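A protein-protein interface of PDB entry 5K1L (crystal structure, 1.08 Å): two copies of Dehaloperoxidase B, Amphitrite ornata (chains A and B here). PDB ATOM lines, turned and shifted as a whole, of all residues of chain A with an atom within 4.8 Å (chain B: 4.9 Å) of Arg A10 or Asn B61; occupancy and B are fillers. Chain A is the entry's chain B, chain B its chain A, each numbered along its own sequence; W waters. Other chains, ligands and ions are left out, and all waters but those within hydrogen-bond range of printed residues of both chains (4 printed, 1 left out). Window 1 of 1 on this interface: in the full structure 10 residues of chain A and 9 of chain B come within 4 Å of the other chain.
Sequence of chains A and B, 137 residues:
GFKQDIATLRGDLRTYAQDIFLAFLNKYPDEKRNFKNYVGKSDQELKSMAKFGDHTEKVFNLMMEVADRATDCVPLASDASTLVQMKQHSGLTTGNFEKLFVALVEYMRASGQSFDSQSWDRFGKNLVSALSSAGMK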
ATOM      1  N   ILE A   6       8.372 -24.518  30.852  1.00  0.00           N
ATOM      2  CA  ILE A   6       9.573 -23.731  31.121  1.00  0.00           C
ATOM      3  C   ILE A   6      10.830 -24.531  30.748  1.00  0.00           C
ATOM      4  O   ILE A   6      11.769 -24.007  30.143  1.00  0.00           O
ATOM      5  CB  ILE A   6       9.584 -23.220  32.572  1.00  0.00           C
ATOM      6  CG1 ILE A   6       8.365 -22.272  32.856  1.00  0.00           C
ATOM      7  CG2 ILE A   6      10.901 -22.521  32.902  1.00  0.00           C
ATOM      8  CD1 ILE A   6       8.147 -21.968  34.363  1.00  0.00           C
ATOM      9  N   ALA A   7      10.861 -25.830  31.126  1.00  0.00           N
ATOM     10  CA  ALA A   7      12.009 -26.727  30.763  1.00  0.00           C
ATOM     11  C   ALA A   7      12.122 -26.953  29.240  1.00  0.00           C
ATOM     12  O   ALA A   7      13.233 -26.914  28.695  1.00  0.00           O
ATOM     13  CB  ALA A   7      11.900 -28.080  31.479  1.00  0.00           C
ATOM     14  N   THR A   8      10.988 -27.150  28.538  1.00  0.00           N
ATOM     15  CA  THR A   8      11.022 -27.282  27.075  1.00  0.00           C
ATOM     16  C   THR A   8      11.642 -26.035  26.427  1.00  0.00           C
ATOM     17  O   THR A   8      12.556 -26.116  25.587  1.00  0.00           O
ATOM     18  CB  THR A   8       9.596 -27.515  26.519  1.00  0.00           C
ATOM     19  OG1 THR A   8       9.103 -28.761  27.033  1.00  0.00           O
ATOM     20  CG2 THR A   8       9.576 -27.525  24.958  1.00  0.00           C
ATOM     21  N   LEU A   9      11.113 -24.871  26.829  1.00  0.00           N
ATOM     22  CA  LEU A   9      11.611 -23.597  26.250  1.00  0.00           C
ATOM     23  C   LEU A   9      13.102 -23.388  26.584  1.00  0.00           C
ATOM     24  O   LEU A   9      13.900 -23.049  25.687  1.00  0.00           O
ATOM     25  CB  LEU A   9      10.731 -22.414  26.724  1.00  0.00           C
ATOM     26  CG  LEU A   9       9.258 -22.429  26.238  1.00  0.00           C
ATOM     27  CD1 LEU A   9       8.446 -21.385  27.010  1.00  0.00           C
ATOM     28  CD2 LEU A   9       9.144 -22.217  24.725  1.00  0.00           C
ATOM     29  N   ARG A  10      13.499 -23.585  27.851  1.00  0.00           N
ATOM     30  CA  ARG A  10      14.928 -23.365  28.173  1.00  0.00           C
ATOM     31  C   ARG A  10      15.859 -24.333  27.465  1.00  0.00           C
ATOM     32  O   ARG A  10      16.993 -23.939  27.135  1.00  0.00           O
ATOM     33  CB  ARG A  10      15.175 -23.399  29.653  1.00  0.00           C
ATOM     34  CG  ARG A  10      14.745 -22.101  30.323  1.00  0.00           C
ATOM     35  CD  ARG A  10      15.351 -22.050  31.740  1.00  0.00           C
ATOM     36  NE  ARG A  10      15.170 -20.796  32.479  1.00  0.00           N
ATOM     37  CZ  ARG A  10      15.842 -19.663  32.247  1.00  0.00           C
ATOM     38  NH1 ARG A  10      16.673 -19.545  31.226  1.00  0.00           N
ATOM     39  NH2 ARG A  10      15.637 -18.629  33.036  1.00  0.00           N
ATOM     40  N   GLY A  11      15.411 -25.563  27.196  1.00  0.00           N
ATOM     41  CA  GLY A  11      16.307 -26.517  26.545  1.00  0.00           C
ATOM     42  C   GLY A  11      16.816 -26.028  25.199  1.00  0.00           C
ATOM     43  O   GLY A  11      17.961 -26.389  24.777  1.00  0.00           O
ATOM     44  N   ASP A  12      15.995 -25.231  24.482  1.00  0.00           N
ATOM     45  CA  ASP A  12      16.403 -24.650  23.196  1.00  0.00           C
ATOM     46  C   ASP A  12      15.996 -23.151  23.141  1.00  0.00           C
ATOM     47  O   ASP A  12      15.284 -22.710  22.216  1.00  0.00           O
ATOM     48  CB  ASP A  12      15.820 -25.420  22.028  1.00  0.00           C
ATOM     49  CG  ASP A  12      16.480 -25.070  20.702  1.00  0.00           C
ATOM     50  OD1 ASP A  12      17.463 -24.265  20.642  1.00  0.00           O
ATOM     51  OD2 ASP A  12      15.988 -25.545  19.647  1.00  0.00           O
ATOM     52  N   LEU A  13      16.451 -22.397  24.149  1.00  0.00           N
ATOM     53  CA  LEU A  13      15.853 -21.059  24.377  1.00  0.00           C
ATOM     54  C   LEU A  13      16.102 -20.111  23.207  1.00  0.00           C
ATOM     55  O   LEU A  13      15.224 -19.307  22.860  1.00  0.00           O
ATOM     56  CB  LEU A  13      16.354 -20.465  25.692  1.00  0.00           C
ATOM     57  CG  LEU A  13      15.571 -19.258  26.195  1.00  0.00           C
ATOM     58  CD1 LEU A  13      14.097 -19.613  26.482  1.00  0.00           C
ATOM     59  CD2 LEU A  13      16.216 -18.715  27.478  1.00  0.00           C
ATOM     60  N   ASN A  61      15.142 -15.193  28.627  1.00  0.00           N
ATOM     61  CA  ASN A  61      15.662 -15.638  29.916  1.00  0.00           C
ATOM     62  C   ASN A  61      14.934 -14.941  31.074  1.00  0.00           C
ATOM     63  O   ASN A  61      14.540 -15.585  32.081  1.00  0.00           O
ATOM     64  CB  ASN A  61      17.203 -15.380  30.014  1.00  0.00           C
ATOM     65  CG  ASN A  61      17.745 -15.627  31.420  1.00  0.00           C
ATOM     66  OD1 ASN A  61      17.607 -16.733  31.954  1.00  0.00           O
ATOM     67  ND2 ASN A  61      18.326 -14.611  31.988  1.00  0.00           N
ATOM     68  N   MET A  64      11.434 -16.329  31.451  1.00  0.00           N
ATOM     69  CA  MET A  64      11.423 -17.631  32.116  1.00  0.00           C
ATOM     70  C   MET A  64      11.706 -17.525  33.638  1.00  0.00           C
ATOM     71  O   MET A  64      11.137 -18.330  34.415  1.00  0.00           O
ATOM     72  CB  MET A  64      12.414 -18.617  31.462  1.00  0.00           C
ATOM     73  CG  MET A  64      12.071 -19.056  30.017  1.00  0.00           C
ATOM     74  SD  MET A  64      10.397 -19.731  29.766  1.00  0.00           S
ATOM     75  CE  MET A  64       9.450 -18.302  29.211  1.00  0.00           C
ATOM     76  N   GLU A  65      12.546 -16.580  34.057  1.00  0.00           N
ATOM     77  CA  GLU A  65      12.748 -16.329  35.522  1.00  0.00           C
ATOM     78  C   GLU A  65      11.438 -15.917  36.180  1.00  0.00           C
ATOM     79  O   GLU A  65      11.071 -16.389  37.271  1.00  0.00           O
ATOM     80  CB  GLU A  65      13.823 -15.229  35.735  1.00  0.00           C
ATOM     81  CG  GLU A  65      15.255 -15.625  35.405  1.00  0.00           C
ATOM     82  CD  GLU A  65      16.276 -14.474  35.536  1.00  0.00           C
ATOM     83  OE1 GLU A  65      17.381 -14.661  36.047  1.00  0.00           O
ATOM     84  OE2 GLU A  65      16.035 -13.389  35.021  1.00  0.00           O
ATOM     85  N   ARG B  10      23.104 -17.636  32.920  1.00  0.00           N
ATOM     86  CA  ARG B  10      21.932 -17.575  32.046  1.00  0.00           C
ATOM     87  C   ARG B  10      21.729 -16.175  31.413  1.00  0.00           C
ATOM     88  O   ARG B  10      21.117 -16.084  30.330  1.00  0.00           O
ATOM     89  CB  ARG B  10      20.649 -18.027  32.787  1.00  0.00           C
ATOM     90  CG  ARG B  10      20.506 -19.516  32.959  1.00  0.00           C
ATOM     91  CD  ARG B  10      19.231 -19.832  33.739  1.00  0.00           C
ATOM     92  NE  ARG B  10      18.884 -21.239  33.598  1.00  0.00           N
ATOM     93  CZ  ARG B  10      18.111 -21.932  34.441  1.00  0.00           C
ATOM     94  NH1 ARG B  10      17.664 -21.430  35.600  1.00  0.00           N
ATOM     95  NH2 ARG B  10      17.818 -23.190  34.124  1.00  0.00           N
ATOM     96  N   LEU B  13      24.365 -16.456  28.129  1.00  0.00           N
ATOM     97  CA  LEU B  13      24.671 -17.876  28.162  1.00  0.00           C
ATOM     98  C   LEU B  13      25.495 -18.392  26.953  1.00  0.00           C
ATOM     99  O   LEU B  13      26.409 -19.226  27.125  1.00  0.00           O
ATOM    100  CB  LEU B  13      23.411 -18.733  28.321  1.00  0.00           C
ATOM    101  CG  LEU B  13      23.622 -20.206  28.705  1.00  0.00           C
ATOM    102  CD1 LEU B  13      24.478 -20.413  29.960  1.00  0.00           C
ATOM    103  CD2 LEU B  13      22.301 -20.892  28.962  1.00  0.00           C
ATOM    104  N   GLU B  57      25.837 -24.130  23.209  1.00  0.00           N
ATOM    105  CA  GLU B  57      24.720 -23.460  23.911  1.00  0.00           C
ATOM    106  C   GLU B  57      23.721 -24.500  24.453  1.00  0.00           C
ATOM    107  O   GLU B  57      23.235 -24.367  25.600  1.00  0.00           O
ATOM    108  CB  GLU B  57      24.051 -22.373  23.058  1.00  0.00           C
ATOM    109  CG  GLU B  57      22.873 -21.624  23.713  1.00  0.00           C
ATOM    110  CD  GLU B  57      22.353 -20.405  22.946  1.00  0.00           C
ATOM    111  OE1 GLU B  57      22.718 -20.233  21.782  1.00  0.00           O
ATOM    112  OE2 GLU B  57      21.539 -19.613  23.495  1.00  0.00           O
ATOM    113  N   LYS B  58      23.332 -25.500  23.635  1.00  0.00           N
ATOM    114  CA  LYS B  58      22.381 -26.513  24.096  1.00  0.00           C
ATOM    115  C   LYS B  58      22.949 -27.325  25.282  1.00  0.00           C
ATOM    116  O   LYS B  58      22.186 -27.663  26.240  1.00  0.00           O
ATOM    117  CB  LYS B  58      21.936 -27.402  22.928  1.00  0.00           C
ATOM    118  CG  LYS B  58      20.915 -26.707  22.019  1.00  0.00           C
ATOM    119  CD  LYS B  58      20.735 -27.471  20.703  1.00  0.00           C
ATOM    120  CE  LYS B  58      19.728 -26.812  19.783  1.00  0.00           C
ATOM    121  NZ  LYS B  58      19.683 -27.409  18.404  1.00  0.00           N
ATOM    122  N   VAL B  59      24.243 -27.624  25.286  1.00  0.00           N
ATOM    123  CA  VAL B  59      24.927 -28.276  26.400  1.00  0.00           C
ATOM    124  C   VAL B  59      24.707 -27.460  27.685  1.00  0.00           C
ATOM    125  O   VAL B  59      24.312 -28.008  28.755  1.00  0.00           O
ATOM    126  CB  VAL B  59      26.443 -28.447  26.131  1.00  0.00           C
ATOM    127  CG1 VAL B  59      27.257 -28.821  27.391  1.00  0.00           C
ATOM    128  CG2 VAL B  59      26.687 -29.455  24.976  1.00  0.00           C
ATOM    129  N   PHE B  60      24.999 -26.140  27.624  1.00  0.00           N
ATOM    130  CA  PHE B  60      24.886 -25.275  28.813  1.00  0.00           C
ATOM    131  C   PHE B  60      23.419 -24.983  29.204  1.00  0.00           C
ATOM    132  O   PHE B  60      23.129 -24.835  30.412  1.00  0.00           O
ATOM    133  CB  PHE B  60      25.760 -24.022  28.656  1.00  0.00           C
ATOM    134  CG  PHE B  60      27.234 -24.288  28.999  1.00  0.00           C
ATOM    135  CD1 PHE B  60      28.074 -24.997  28.105  1.00  0.00           C
ATOM    136  CD2 PHE B  60      27.778 -23.857  30.216  1.00  0.00           C
ATOM    137  CE1 PHE B  60      29.387 -25.292  28.457  1.00  0.00           C
ATOM    138  CE2 PHE B  60      29.114 -24.116  30.519  1.00  0.00           C
ATOM    139  CZ  PHE B  60      29.911 -24.824  29.631  1.00  0.00           C
ATOM    140  N   ASN B  61      22.484 -24.948  28.239  1.00  0.00           N
ATOM    141  CA  ASN B  61      21.061 -24.822  28.608  1.00  0.00           C
ATOM    142  C   ASN B  61      20.687 -25.988  29.565  1.00  0.00           C
ATOM    143  O   ASN B  61      20.048 -25.767  30.619  1.00  0.00           O
ATOM    144  CB  ASN B  61      20.159 -24.921  27.344  1.00  0.00           C
ATOM    145  CG  ASN B  61      20.185 -23.672  26.431  1.00  0.00           C
ATOM    146  OD1 ASN B  61      20.521 -22.573  26.858  1.00  0.00           O
ATOM    147  ND2 ASN B  61      19.710 -23.844  25.172  1.00  0.00           N
ATOM    148  N   LEU B  62      21.074 -27.230  29.181  1.00  0.00           N
ATOM    149  CA  LEU B  62      20.791 -28.397  30.015  1.00  0.00           C
ATOM    150  C   LEU B  62      21.610 -28.400  31.328  1.00  0.00           C
ATOM    151  O   LEU B  62      21.047 -28.705  32.404  1.00  0.00           O
ATOM    152  CB  LEU B  62      21.023 -29.707  29.225  1.00  0.00           C
ATOM    153  CG  LEU B  62      20.695 -30.991  29.987  1.00  0.00           C
ATOM    154  CD1 LEU B  62      19.250 -31.021  30.501  1.00  0.00           C
ATOM    155  CD2 LEU B  62      20.941 -32.195  29.086  1.00  0.00           C
ATOM    156  N   MET B  63      22.895 -28.032  31.252  1.00  0.00           N
ATOM    157  CA  MET B  63      23.723 -28.022  32.484  1.00  0.00           C
ATOM    158  C   MET B  63      23.075 -27.069  33.536  1.00  0.00           C
ATOM    159  O   MET B  63      23.063 -27.410  34.735  1.00  0.00           O
ATOM    160  CB  MET B  63      25.167 -27.558  32.184  1.00  0.00           C
ATOM    161  CG  MET B  63      26.121 -27.742  33.342  1.00  0.00           C
ATOM    162  SD  MET B  63      27.716 -26.857  33.265  1.00  0.00           S
ATOM    163  CE  MET B  63      28.444 -27.685  31.856  1.00  0.00           C
ATOM    164  N   MET B  64      22.581 -25.901  33.086  1.00  0.00           N
ATOM    165  CA  MET B  64      21.984 -24.940  34.031  1.00  0.00           C
ATOM    166  C   MET B  64      20.677 -25.493  34.640  1.00  0.00           C
ATOM    167  O   MET B  64      20.385 -25.243  35.818  1.00  0.00           O
ATOM    168  CB  MET B  64      21.770 -23.560  33.394  1.00  0.00           C
ATOM    169  CG  MET B  64      23.061 -22.807  33.039  1.00  0.00           C
ATOM    170  SD  MET B  64      24.233 -22.555  34.413  1.00  0.00           S
ATOM    171  CE  MET B  64      25.384 -23.898  34.197  1.00  0.00           C
ATOM    172  N   GLU B  65      19.883 -26.235  33.843  1.00  0.00           N
ATOM    173  CA  GLU B  65      18.692 -26.904  34.395  1.00  0.00           C
ATOM    174  C   GLU B  65      19.063 -27.970  35.455  1.00  0.00           C
ATOM    175  O   GLU B  65      18.386 -28.084  36.489  1.00  0.00           O
ATOM    176  CB  GLU B  65      17.848 -27.535  33.271  1.00  0.00           C
ATOM    177  CG  GLU B  65      17.170 -26.501  32.342  1.00  0.00           C
ATOM    178  CD  GLU B  65      16.309 -27.210  31.378  1.00  0.00           C
ATOM    179  OE1 GLU B  65      15.202 -27.584  31.691  1.00  0.00           O
ATOM    180  OE2 GLU B  65      16.859 -27.482  30.309  1.00  0.00           O
HETATM  181  O   HOH W   1      18.318 -22.016  28.791  1.00  0.00           O
HETATM  182  O   HOH W   2      19.306 -22.704  22.372  1.00  0.00           O
HETATM  183  O   HOH W   3      19.459 -28.451  25.851  1.00  0.00           O
HETATM  184  O   HOH W   4      15.258 -28.884  29.007  1.00  0.00           O
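ND2 of Asn B61 sits close to O of Arg A10, 3.4 Å away.
ND2 of Asn B61 sits at hydrogen-bond distance from O of Gly A11.
The side-chain amide oxygen of Asn B61 sits close to the backbone carbonyl oxygen of Glu B57, at 3.5 Å.
The guanidinium group (NH2) of Arg A10 lies within hydrogen-bond range of the side-chain amide oxygen (OD1) of Asn A61.
Glu B65 touches Ala A7.
Arg A10 touches Arg B10 (NH1 to CD, 3.6 Å).
Gly A11 touches Glu B65.
Asp A12 touches Lys B58 (OD1 to CE, 3.5 Å).
Asp A12 touches Asn B61.
Asn B61 touches Leu A13 (ND2 to N, 3.7 Å).
Arg B10 touches Asn A61.
Of the printed residues of chain B, Arg A10 touches Arg B10 and Asn B61.
Of the printed residues of chain B, Gly A11 touches Asn B61 and Glu B65.
Printed residues of chain A within 4 Å of Arg B10: Arg A10 and Asn A61.
Printed residues of chain B within 4 Å of Asn A61: Arg B10.
Of the printed residues of chain A, Lys B58 touches Asp A12.
Of the printed residues of chain B, Leu A13 touches Asn B61 (3.7 Å).
The nearest printed residue of chain A that does not touch Asn B61 is Leu A9 (5.9 Å).
The nearest printed residue of chain A that does not touch Lys B58 is Gly A11 (4.1 Å).
Hydrophobic or aromatic side chains of chain A within 4 Å of the printed part of chain B: Ala A7.
Along chain A the printed residues that touch a printed residue of chain B span positions 7 to 61.
Among the printed residues, 9 pairs touch across the chains.
Among the printed residues, no Asp or Glu carboxylate lies within 4 Å of a Lys or Arg side-chain nitrogen of the other chain.
Arg A10 touches its own counterpart, Arg B10.
Arg A10 touches Asn B61, and with the chains exchanged Asn A61 touches Arg B10.
Leu A13 touches Asn B61, but with the chains exchanged Asn A61 does not touch Leu B13 (6.9 Å).
5 positions are printed for both chains.
Of the 9 pairs that touch across the chains among the printed residues, 3 have their exchanged pair printed and touching as well.
Water W4 bridges the side-chain carboxylate (OE2) of Glu B65 (2.5 Å) and the backbone carbonyl oxygen (O) of Ala A7 (2.8 Å).
Water W3 bridges O of Gly A11 (2.8 Å) and O of Lys B58 (2.9 Å).
Water W1 lies within hydrogen-bond range of O of Arg A10 and OD1 of Asn B61.
Water W2 lies within hydrogen-bond range of the side-chain carboxylate (OD1) of Asp A12 (3.0 Å), the side-chain amide nitrogen (ND2) of Asn B61 (3.1 Å) and the backbone NH (N) of Leu A13 (3.4 Å).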
